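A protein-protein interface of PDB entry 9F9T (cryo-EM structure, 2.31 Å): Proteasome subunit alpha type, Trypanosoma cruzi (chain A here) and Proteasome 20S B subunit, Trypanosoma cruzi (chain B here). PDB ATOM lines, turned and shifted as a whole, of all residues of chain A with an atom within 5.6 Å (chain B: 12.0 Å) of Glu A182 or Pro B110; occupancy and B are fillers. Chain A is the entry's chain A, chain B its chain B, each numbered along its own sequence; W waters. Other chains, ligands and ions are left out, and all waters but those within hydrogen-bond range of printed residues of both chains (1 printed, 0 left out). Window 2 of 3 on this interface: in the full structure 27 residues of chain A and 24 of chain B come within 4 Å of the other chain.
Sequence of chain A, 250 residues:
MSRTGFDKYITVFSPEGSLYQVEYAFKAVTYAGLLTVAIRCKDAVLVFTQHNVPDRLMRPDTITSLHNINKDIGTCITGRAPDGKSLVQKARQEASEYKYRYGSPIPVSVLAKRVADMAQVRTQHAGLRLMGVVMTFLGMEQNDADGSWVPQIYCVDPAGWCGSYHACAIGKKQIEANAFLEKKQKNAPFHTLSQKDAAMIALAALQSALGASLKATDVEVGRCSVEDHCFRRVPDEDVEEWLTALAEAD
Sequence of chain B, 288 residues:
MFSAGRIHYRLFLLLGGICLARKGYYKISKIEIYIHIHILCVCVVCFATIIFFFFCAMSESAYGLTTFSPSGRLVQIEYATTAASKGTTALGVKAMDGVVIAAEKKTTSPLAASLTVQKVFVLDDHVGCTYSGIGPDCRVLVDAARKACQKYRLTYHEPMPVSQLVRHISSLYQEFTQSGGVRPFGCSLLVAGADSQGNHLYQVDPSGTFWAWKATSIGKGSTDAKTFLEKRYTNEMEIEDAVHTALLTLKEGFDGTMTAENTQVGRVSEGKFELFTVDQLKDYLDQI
The side-chain amide nitrogen (NE2) of Gln A185 lies within hydrogen-bond range of the backbone carbonyl oxygen (O) of Pro B110 (2.8 Å).
ND1 of His A166 sits at hydrogen-bond distance from O of Ala B112.
O of Leu B111 sits at hydrogen-bond distance from N of His A166 (2.8 Å).
Of the 16 printed residues of chain B, 5 touch a printed residue of chain A.
Hydrophobic or aromatic side chains of chain B that line the printed part of chain A: Pro B110, Leu B111 and Ala B113.
Of the 11 printed residues of chain A, 4 touch a printed residue of chain B.
Printed residues of chain A that touch a printed residue of chain B: His A166, Asn A178, Glu A182 and Gln A185.
Among the printed residues, no Asp or Glu carboxylate lies within 4 Å of a Lys or Arg side-chain nitrogen of the other chain.
Asn A178 touches one residue of chain B.
No residue of chain B comes within 4 Å of Ala A179.
Of the printed residues of chain B, Glu A182 touches Ser B109 (3.7 Å) and Pro B110 (3.9 Å).
No residue of chain B comes within 4 Å of Lys A183.
Gln A185 touches two residues of chain B.
No residue of chain B comes within 4 Å of Lys A186.
Of the printed residues of chain A, Ser B109 touches Glu A182 (3.7 Å).
Pro B110 touches just these residues of chain A: His A166, Glu A182 and Gln A185.
Printed residues of chain A within 4 Å of Leu B111: His A166, Asn A178 and Gln A185.
Printed residues of chain A within 4 Å of Ala B112: His A166 (3.5 Å).
Printed residues of chain A within 4 Å of Ala B113: His A166 (3.6 Å).
The nearest printed residue of chain A that does not touch Pro B110 is Lys A186 (5.7 Å).
The nearest printed residue of chain A that does not touch Ala B113 is Gln A185 (7.5 Å).
Among the printed residues, merely in contact across the chains: Asn A178 with Leu B111 (3.4 Å), Gln A185 with Leu B111 (3.5 Å), His A166 with Ala B113 (3.6 Å), Glu A182 with Ser B109 (3.7 Å), His A166 with Pro B110 (3.9 Å) and Glu A182 with Pro B110 (3.9 Å).
Water W1 lies within hydrogen-bond range of O of Thr B108 and OE1 of Glu A182.
The side-chain hydroxyl of Ser B109 sits at hydrogen-bond distance from the backbone NH of Leu B111 (2.7 Å).
The side-chain hydroxyl (OG1) of Thr B107 sits at hydrogen-bond distance from the backbone carbonyl oxygen (O) of Ser B109.
O of Ala B113 lies within hydrogen-bond range of OG1 of Thr B116 (3.3 Å).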
ATOM      1  N   HIS A 166       1.135   9.840  -9.582  1.00  0.00           N
ATOM      2  CA  HIS A 166       2.214  10.832  -9.638  1.00  0.00           C
ATOM      3  C   HIS A 166       1.749  12.020 -10.487  1.00  0.00           C
ATOM      4  O   HIS A 166       2.138  13.160 -10.264  1.00  0.00           O
ATOM      5  CB  HIS A 166       3.521  10.206 -10.151  1.00  0.00           C
ATOM      6  CG  HIS A 166       4.023   9.063  -9.296  1.00  0.00           C
ATOM      7  ND1 HIS A 166       4.056   7.749  -9.718  1.00  0.00           N
ATOM      8  CD2 HIS A 166       4.516   9.048  -8.026  1.00  0.00           C
ATOM      9  CE1 HIS A 166       4.536   6.978  -8.747  1.00  0.00           C
ATOM     10  NE2 HIS A 166       4.833   7.734  -7.705  1.00  0.00           N
ATOM     11  N   ALA A 177      -2.981  13.458 -23.534  1.00  0.00           N
ATOM     12  CA  ALA A 177      -2.318  14.278 -22.534  1.00  0.00           C
ATOM     13  C   ALA A 177      -1.535  13.413 -21.544  1.00  0.00           C
ATOM     14  O   ALA A 177      -0.497  13.834 -21.025  1.00  0.00           O
ATOM     15  CB  ALA A 177      -3.350  15.095 -21.799  1.00  0.00           C
ATOM     16  N   ASN A 178      -2.104  12.241 -21.236  1.00  0.00           N
ATOM     17  CA  ASN A 178      -1.467  11.256 -20.382  1.00  0.00           C
ATOM     18  C   ASN A 178      -0.212  10.698 -21.052  1.00  0.00           C
ATOM     19  O   ASN A 178       0.750  10.413 -20.347  1.00  0.00           O
ATOM     20  CB  ASN A 178      -2.421  10.135 -19.975  1.00  0.00           C
ATOM     21  CG  ASN A 178      -3.146  10.398 -18.661  1.00  0.00           C
ATOM     22  OD1 ASN A 178      -2.579  10.869 -17.677  1.00  0.00           O
ATOM     23  ND2 ASN A 178      -4.425  10.092 -18.622  1.00  0.00           N
ATOM     24  N   ALA A 179      -0.212  10.548 -22.390  1.00  0.00           N
ATOM     25  CA  ALA A 179       0.957  10.117 -23.158  1.00  0.00           C
ATOM     26  C   ALA A 179       2.041  11.182 -23.138  1.00  0.00           C
ATOM     27  O   ALA A 179       3.225  10.886 -23.043  1.00  0.00           O
ATOM     28  CB  ALA A 179       0.569   9.850 -24.585  1.00  0.00           C
ATOM     29  N   PHE A 180       1.644  12.442 -23.213  1.00  0.00           N
ATOM     30  CA  PHE A 180       2.612  13.510 -23.132  1.00  0.00           C
ATOM     31  C   PHE A 180       3.314  13.533 -21.771  1.00  0.00           C
ATOM     32  O   PHE A 180       4.483  13.903 -21.702  1.00  0.00           O
ATOM     33  CB  PHE A 180       1.904  14.825 -23.472  1.00  0.00           C
ATOM     34  CG  PHE A 180       2.800  16.041 -23.414  1.00  0.00           C
ATOM     35  CD1 PHE A 180       3.202  16.668 -24.579  1.00  0.00           C
ATOM     36  CD2 PHE A 180       3.232  16.542 -22.201  1.00  0.00           C
ATOM     37  CE1 PHE A 180       4.047  17.774 -24.539  1.00  0.00           C
ATOM     38  CE2 PHE A 180       4.085  17.641 -22.151  1.00  0.00           C
ATOM     39  CZ  PHE A 180       4.483  18.263 -23.322  1.00  0.00           C
ATOM     40  N   LEU A 181       2.580  13.234 -20.685  1.00  0.00           N
ATOM     41  CA  LEU A 181       3.143  13.216 -19.341  1.00  0.00           C
ATOM     42  C   LEU A 181       4.017  11.980 -19.155  1.00  0.00           C
ATOM     43  O   LEU A 181       4.936  12.021 -18.340  1.00  0.00           O
ATOM     44  CB  LEU A 181       2.039  13.155 -18.279  1.00  0.00           C
ATOM     45  CG  LEU A 181       1.117  14.360 -18.142  1.00  0.00           C
ATOM     46  CD1 LEU A 181      -0.061  13.987 -17.249  1.00  0.00           C
ATOM     47  CD2 LEU A 181       1.867  15.577 -17.612  1.00  0.00           C
ATOM     48  N   GLU A 182       3.654  10.863 -19.813  1.00  0.00           N
ATOM     49  CA  GLU A 182       4.460   9.645 -19.778  1.00  0.00           C
ATOM     50  C   GLU A 182       5.845   9.916 -20.377  1.00  0.00           C
ATOM     51  O   GLU A 182       6.836   9.487 -19.807  1.00  0.00           O
ATOM     52  CB  GLU A 182       3.766   8.478 -20.498  1.00  0.00           C
ATOM     53  CG  GLU A 182       2.925   7.580 -19.596  1.00  0.00           C
ATOM     54  CD  GLU A 182       1.981   6.654 -20.361  1.00  0.00           C
ATOM     55  OE1 GLU A 182       0.733   6.772 -20.203  1.00  0.00           O
ATOM     56  OE2 GLU A 182       2.490   5.822 -21.147  1.00  0.00           O
ATOM     57  N   LYS A 183       5.898  10.624 -21.514  1.00  0.00           N
ATOM     58  CA  LYS A 183       7.157  10.984 -22.157  1.00  0.00           C
ATOM     59  C   LYS A 183       8.047  11.810 -21.244  1.00  0.00           C
ATOM     60  O   LYS A 183       9.263  11.652 -21.272  1.00  0.00           O
ATOM     61  CB  LYS A 183       6.981  11.862 -23.395  1.00  0.00           C
ATOM     62  CG  LYS A 183       7.515  11.278 -24.689  1.00  0.00           C
ATOM     63  CD  LYS A 183       7.773  12.342 -25.744  1.00  0.00           C
ATOM     64  CE  LYS A 183       7.923  11.763 -27.138  1.00  0.00           C
ATOM     65  NZ  LYS A 183       6.741  10.953 -27.532  1.00  0.00           N
ATOM     66  N   LYS A 184       7.440  12.739 -20.510  1.00  0.00           N
ATOM     67  CA  LYS A 184       8.191  13.737 -19.769  1.00  0.00           C
ATOM     68  C   LYS A 184       8.502  13.206 -18.375  1.00  0.00           C
ATOM     69  O   LYS A 184       9.205  13.856 -17.604  1.00  0.00           O
ATOM     70  CB  LYS A 184       7.383  15.032 -19.687  1.00  0.00           C
ATOM     71  CG  LYS A 184       7.293  15.829 -20.974  1.00  0.00           C
ATOM     72  CD  LYS A 184       8.056  17.123 -20.923  1.00  0.00           C
ATOM     73  CE  LYS A 184       7.843  17.982 -22.154  1.00  0.00           C
ATOM     74  NZ  LYS A 184       8.940  17.832 -23.132  1.00  0.00           N
ATOM     75  N   GLN A 185       7.964  12.028 -18.053  1.00  0.00           N
ATOM     76  CA  GLN A 185       8.289  11.344 -16.812  1.00  0.00           C
ATOM     77  C   GLN A 185       9.675  10.710 -16.930  1.00  0.00           C
ATOM     78  O   GLN A 185      10.375  10.563 -15.924  1.00  0.00           O
ATOM     79  CB  GLN A 185       7.214  10.297 -16.529  1.00  0.00           C
ATOM     80  CG  GLN A 185       7.211   9.717 -15.111  1.00  0.00           C
ATOM     81  CD  GLN A 185       6.250   8.547 -15.081  1.00  0.00           C
ATOM     82  OE1 GLN A 185       6.218   7.722 -15.996  1.00  0.00           O
ATOM     83  NE2 GLN A 185       5.417   8.504 -14.061  1.00  0.00           N
ATOM     84  N   LYS A 186      10.056  10.367 -18.175  1.00  0.00           N
ATOM     85  CA  LYS A 186      11.231   9.555 -18.459  1.00  0.00           C
ATOM     86  C   LYS A 186      12.513  10.361 -18.252  1.00  0.00           C
ATOM     87  O   LYS A 186      13.558   9.796 -17.927  1.00  0.00           O
ATOM     88  CB  LYS A 186      11.143   8.987 -19.877  1.00  0.00           C
ATOM     89  CG  LYS A 186      10.126   7.867 -20.037  1.00  0.00           C
ATOM     90  CD  LYS A 186      10.353   7.009 -21.272  1.00  0.00           C
ATOM     91  CE  LYS A 186       9.853   5.585 -21.112  1.00  0.00           C
ATOM     92  NZ  LYS A 186       8.376   5.493 -21.238  1.00  0.00           N
ATOM     93  N   LYS B 105      -0.192  -7.131  -9.255  1.00  0.00           N
ATOM     94  CA  LYS B 105      -0.726  -5.773  -9.266  1.00  0.00           C
ATOM     95  C   LYS B 105      -0.045  -4.977 -10.351  1.00  0.00           C
ATOM     96  O   LYS B 105       0.874  -4.240 -10.042  1.00  0.00           O
ATOM     97  CB  LYS B 105      -0.489  -4.936  -8.000  1.00  0.00           C
ATOM     98  CG  LYS B 105       0.803  -5.176  -7.240  1.00  0.00           C
ATOM     99  CD  LYS B 105       0.834  -4.565  -5.820  1.00  0.00           C
ATOM    100  CE  LYS B 105       1.492  -3.207  -5.787  1.00  0.00           C
ATOM    101  NZ  LYS B 105       1.568  -2.664  -4.413  1.00  0.00           N
ATOM    102  N   LYS B 106      -0.485  -5.133 -11.594  1.00  0.00           N
ATOM    103  CA  LYS B 106       0.012  -4.251 -12.631  1.00  0.00           C
ATOM    104  C   LYS B 106      -0.907  -3.035 -12.698  1.00  0.00           C
ATOM    105  O   LYS B 106      -2.133  -3.167 -12.673  1.00  0.00           O
ATOM    106  CB  LYS B 106       0.125  -4.980 -13.975  1.00  0.00           C
ATOM    107  CG  LYS B 106       1.157  -6.107 -14.025  1.00  0.00           C
ATOM    108  CD  LYS B 106       1.594  -6.501 -15.422  1.00  0.00           C
ATOM    109  CE  LYS B 106       0.449  -6.882 -16.342  1.00  0.00           C
ATOM    110  NZ  LYS B 106       0.841  -6.790 -17.771  1.00  0.00           N
ATOM    111  N   THR B 107      -0.270  -1.858 -12.798  1.00  0.00           N
ATOM    112  CA  THR B 107      -0.908  -0.600 -13.172  1.00  0.00           C
ATOM    113  C   THR B 107      -1.016  -0.442 -14.701  1.00  0.00           C
ATOM    114  O   THR B 107      -0.265  -1.029 -15.485  1.00  0.00           O
ATOM    115  CB  THR B 107      -0.125   0.566 -12.547  1.00  0.00           C
ATOM    116  OG1 THR B 107       1.245   0.455 -12.947  1.00  0.00           O
ATOM    117  CG2 THR B 107      -0.217   0.592 -11.038  1.00  0.00           C
ATOM    118  N   THR B 108      -1.950   0.413 -15.122  1.00  0.00           N
ATOM    119  CA  THR B 108      -2.197   0.667 -16.532  1.00  0.00           C
ATOM    120  C   THR B 108      -1.110   1.581 -17.106  1.00  0.00           C
ATOM    121  O   THR B 108      -0.731   1.420 -18.267  1.00  0.00           O
ATOM    122  CB  THR B 108      -3.615   1.228 -16.736  1.00  0.00           C
ATOM    123  OG1 THR B 108      -3.701   2.527 -16.147  1.00  0.00           O
ATOM    124  CG2 THR B 108      -4.689   0.338 -16.144  1.00  0.00           C
ATOM    125  N   SER B 109      -0.638   2.549 -16.301  1.00  0.00           N
ATOM    126  CA  SER B 109       0.448   3.435 -16.700  1.00  0.00           C
ATOM    127  C   SER B 109       1.456   3.597 -15.568  1.00  0.00           C
ATOM    128  O   SER B 109       1.117   3.429 -14.395  1.00  0.00           O
ATOM    129  CB  SER B 109      -0.074   4.797 -17.127  1.00  0.00           C
ATOM    130  OG  SER B 109       0.178   5.810 -16.155  1.00  0.00           O
ATOM    131  N   PRO B 110       2.696   4.012 -15.900  1.00  0.00           N
ATOM    132  CA  PRO B 110       3.680   4.451 -14.903  1.00  0.00           C
ATOM    133  C   PRO B 110       3.407   5.781 -14.193  1.00  0.00           C
ATOM    134  O   PRO B 110       4.094   6.130 -13.241  1.00  0.00           O
ATOM    135  CB  PRO B 110       4.960   4.627 -15.719  1.00  0.00           C
ATOM    136  CG  PRO B 110       4.471   4.923 -17.132  1.00  0.00           C
ATOM    137  CD  PRO B 110       3.193   4.122 -17.281  1.00  0.00           C
ATOM    138  N   LEU B 111       2.371   6.502 -14.647  1.00  0.00           N
ATOM    139  CA  LEU B 111       1.834   7.649 -13.934  1.00  0.00           C
ATOM    140  C   LEU B 111       1.105   7.276 -12.630  1.00  0.00           C
ATOM    141  O   LEU B 111       1.033   8.069 -11.694  1.00  0.00           O
ATOM    142  CB  LEU B 111       0.879   8.337 -14.893  1.00  0.00           C
ATOM    143  CG  LEU B 111       1.548   8.995 -16.096  1.00  0.00           C
ATOM    144  CD1 LEU B 111       0.488   9.651 -17.011  1.00  0.00           C
ATOM    145  CD2 LEU B 111       2.622   9.972 -15.622  1.00  0.00           C
ATOM    146  N   ALA B 112       0.474   6.110 -12.603  1.00  0.00           N
ATOM    147  CA  ALA B 112      -0.048   5.563 -11.377  1.00  0.00           C
ATOM    148  C   ALA B 112       1.077   5.276 -10.385  1.00  0.00           C
ATOM    149  O   ALA B 112       2.205   4.970 -10.756  1.00  0.00           O
ATOM    150  CB  ALA B 112      -0.801   4.313 -11.695  1.00  0.00           C
ATOM    151  N   ALA B 113       0.716   5.372  -9.111  1.00  0.00           N
ATOM    152  CA  ALA B 113       1.589   5.035  -8.001  1.00  0.00           C
ATOM    153  C   ALA B 113       1.353   3.574  -7.623  1.00  0.00           C
ATOM    154  O   ALA B 113       0.250   3.174  -7.260  1.00  0.00           O
ATOM    155  CB  ALA B 113       1.343   5.982  -6.860  1.00  0.00           C
ATOM    156  N   SER B 114       2.405   2.785  -7.767  1.00  0.00           N
ATOM    157  CA  SER B 114       2.346   1.349  -7.611  1.00  0.00           C
ATOM    158  C   SER B 114       2.121   0.981  -6.147  1.00  0.00           C
ATOM    159  O   SER B 114       1.320   0.098  -5.851  1.00  0.00           O
ATOM    160  CB  SER B 114       3.615   0.761  -8.141  1.00  0.00           C
ATOM    161  OG  SER B 114       3.824   1.197  -9.489  1.00  0.00           O
ATOM    162  N   LEU B 115       2.799   1.698  -5.256  1.00  0.00           N
ATOM    163  CA  LEU B 115       2.889   1.335  -3.861  1.00  0.00           C
ATOM    164  C   LEU B 115       1.528   1.373  -3.171  1.00  0.00           C
ATOM    165  O   LEU B 115       1.342   0.718  -2.149  1.00  0.00           O
ATOM    166  CB  LEU B 115       3.870   2.314  -3.203  1.00  0.00           C
ATOM    167  CG  LEU B 115       4.113   2.135  -1.698  1.00  0.00           C
ATOM    168  CD1 LEU B 115       4.846   0.823  -1.405  1.00  0.00           C
ATOM    169  CD2 LEU B 115       4.880   3.325  -1.118  1.00  0.00           C
ATOM    170  N   THR B 116       0.570   2.140  -3.701  1.00  0.00           N
ATOM    171  CA  THR B 116      -0.711   2.290  -3.026  1.00  0.00           C
ATOM    172  C   THR B 116      -1.723   1.242  -3.496  1.00  0.00           C
ATOM    173  O   THR B 116      -2.725   1.056  -2.819  1.00  0.00           O
ATOM    174  CB  THR B 116      -1.264   3.727  -3.148  1.00  0.00           C
ATOM    175  OG1 THR B 116      -1.278   4.148  -4.522  1.00  0.00           O
ATOM    176  CG2 THR B 116      -0.469   4.704  -2.299  1.00  0.00           C
ATOM    177  N   VAL B 117      -1.478   0.546  -4.607  1.00  0.00           N
ATOM    178  CA  VAL B 117      -2.394  -0.503  -5.046  1.00  0.00           C
ATOM    179  C   VAL B 117      -2.323  -1.694  -4.083  1.00  0.00           C
ATOM    180  O   VAL B 117      -1.296  -2.310  -3.925  1.00  0.00           O
ATOM    181  CB  VAL B 117      -2.121  -0.970  -6.496  1.00  0.00           C
ATOM    182  CG1 VAL B 117      -3.056  -2.109  -6.856  1.00  0.00           C
ATOM    183  CG2 VAL B 117      -2.183   0.158  -7.542  1.00  0.00           C
ATOM    184  N   THR B 259       8.299  -7.911 -10.800  1.00  0.00           N
ATOM    185  CA  THR B 259       9.144  -7.091  -9.947  1.00  0.00           C
ATOM    186  C   THR B 259       8.571  -7.184  -8.534  1.00  0.00           C
ATOM    187  O   THR B 259       7.542  -7.834  -8.366  1.00  0.00           O
ATOM    188  CB  THR B 259       9.217  -5.645 -10.488  1.00  0.00           C
ATOM    189  OG1 THR B 259       9.171  -5.589 -11.914  1.00  0.00           O
ATOM    190  CG2 THR B 259      10.486  -4.929 -10.072  1.00  0.00           C
ATOM    191  N   GLU B 261       7.419  -4.562  -7.210  1.00  0.00           N
ATOM    192  CA  GLU B 261       6.483  -3.452  -7.259  1.00  0.00           C
ATOM    193  C   GLU B 261       5.220  -3.775  -8.068  1.00  0.00           C
ATOM    194  O   GLU B 261       4.353  -2.906  -8.172  1.00  0.00           O
ATOM    195  CB  GLU B 261       7.141  -2.213  -7.891  1.00  0.00           C
ATOM    196  CG  GLU B 261       8.265  -1.583  -7.068  1.00  0.00           C
ATOM    197  CD  GLU B 261       8.822  -0.306  -7.692  1.00  0.00           C
ATOM    198  OE1 GLU B 261      10.049  -0.252  -7.940  1.00  0.00           O
ATOM    199  OE2 GLU B 261       8.028   0.635  -7.953  1.00  0.00           O
ATOM    200  N   ASN B 262       5.107  -4.961  -8.686  1.00  0.00           N
ATOM    201  CA  ASN B 262       3.876  -5.299  -9.396  1.00  0.00           C
ATOM    202  C   ASN B 262       3.367  -6.694  -8.978  1.00  0.00           C
ATOM    203  O   ASN B 262       2.584  -7.351  -9.683  1.00  0.00           O
ATOM    204  CB  ASN B 262       4.051  -5.145 -10.909  1.00  0.00           C
ATOM    205  CG  ASN B 262       5.083  -6.119 -11.439  1.00  0.00           C
ATOM    206  OD1 ASN B 262       5.521  -6.999 -10.694  1.00  0.00           O
ATOM    207  ND2 ASN B 262       5.471  -5.951 -12.700  1.00  0.00           N
HETATM  208  O   HOH W   1      -1.105   3.852 -20.079  1.00  0.00           O
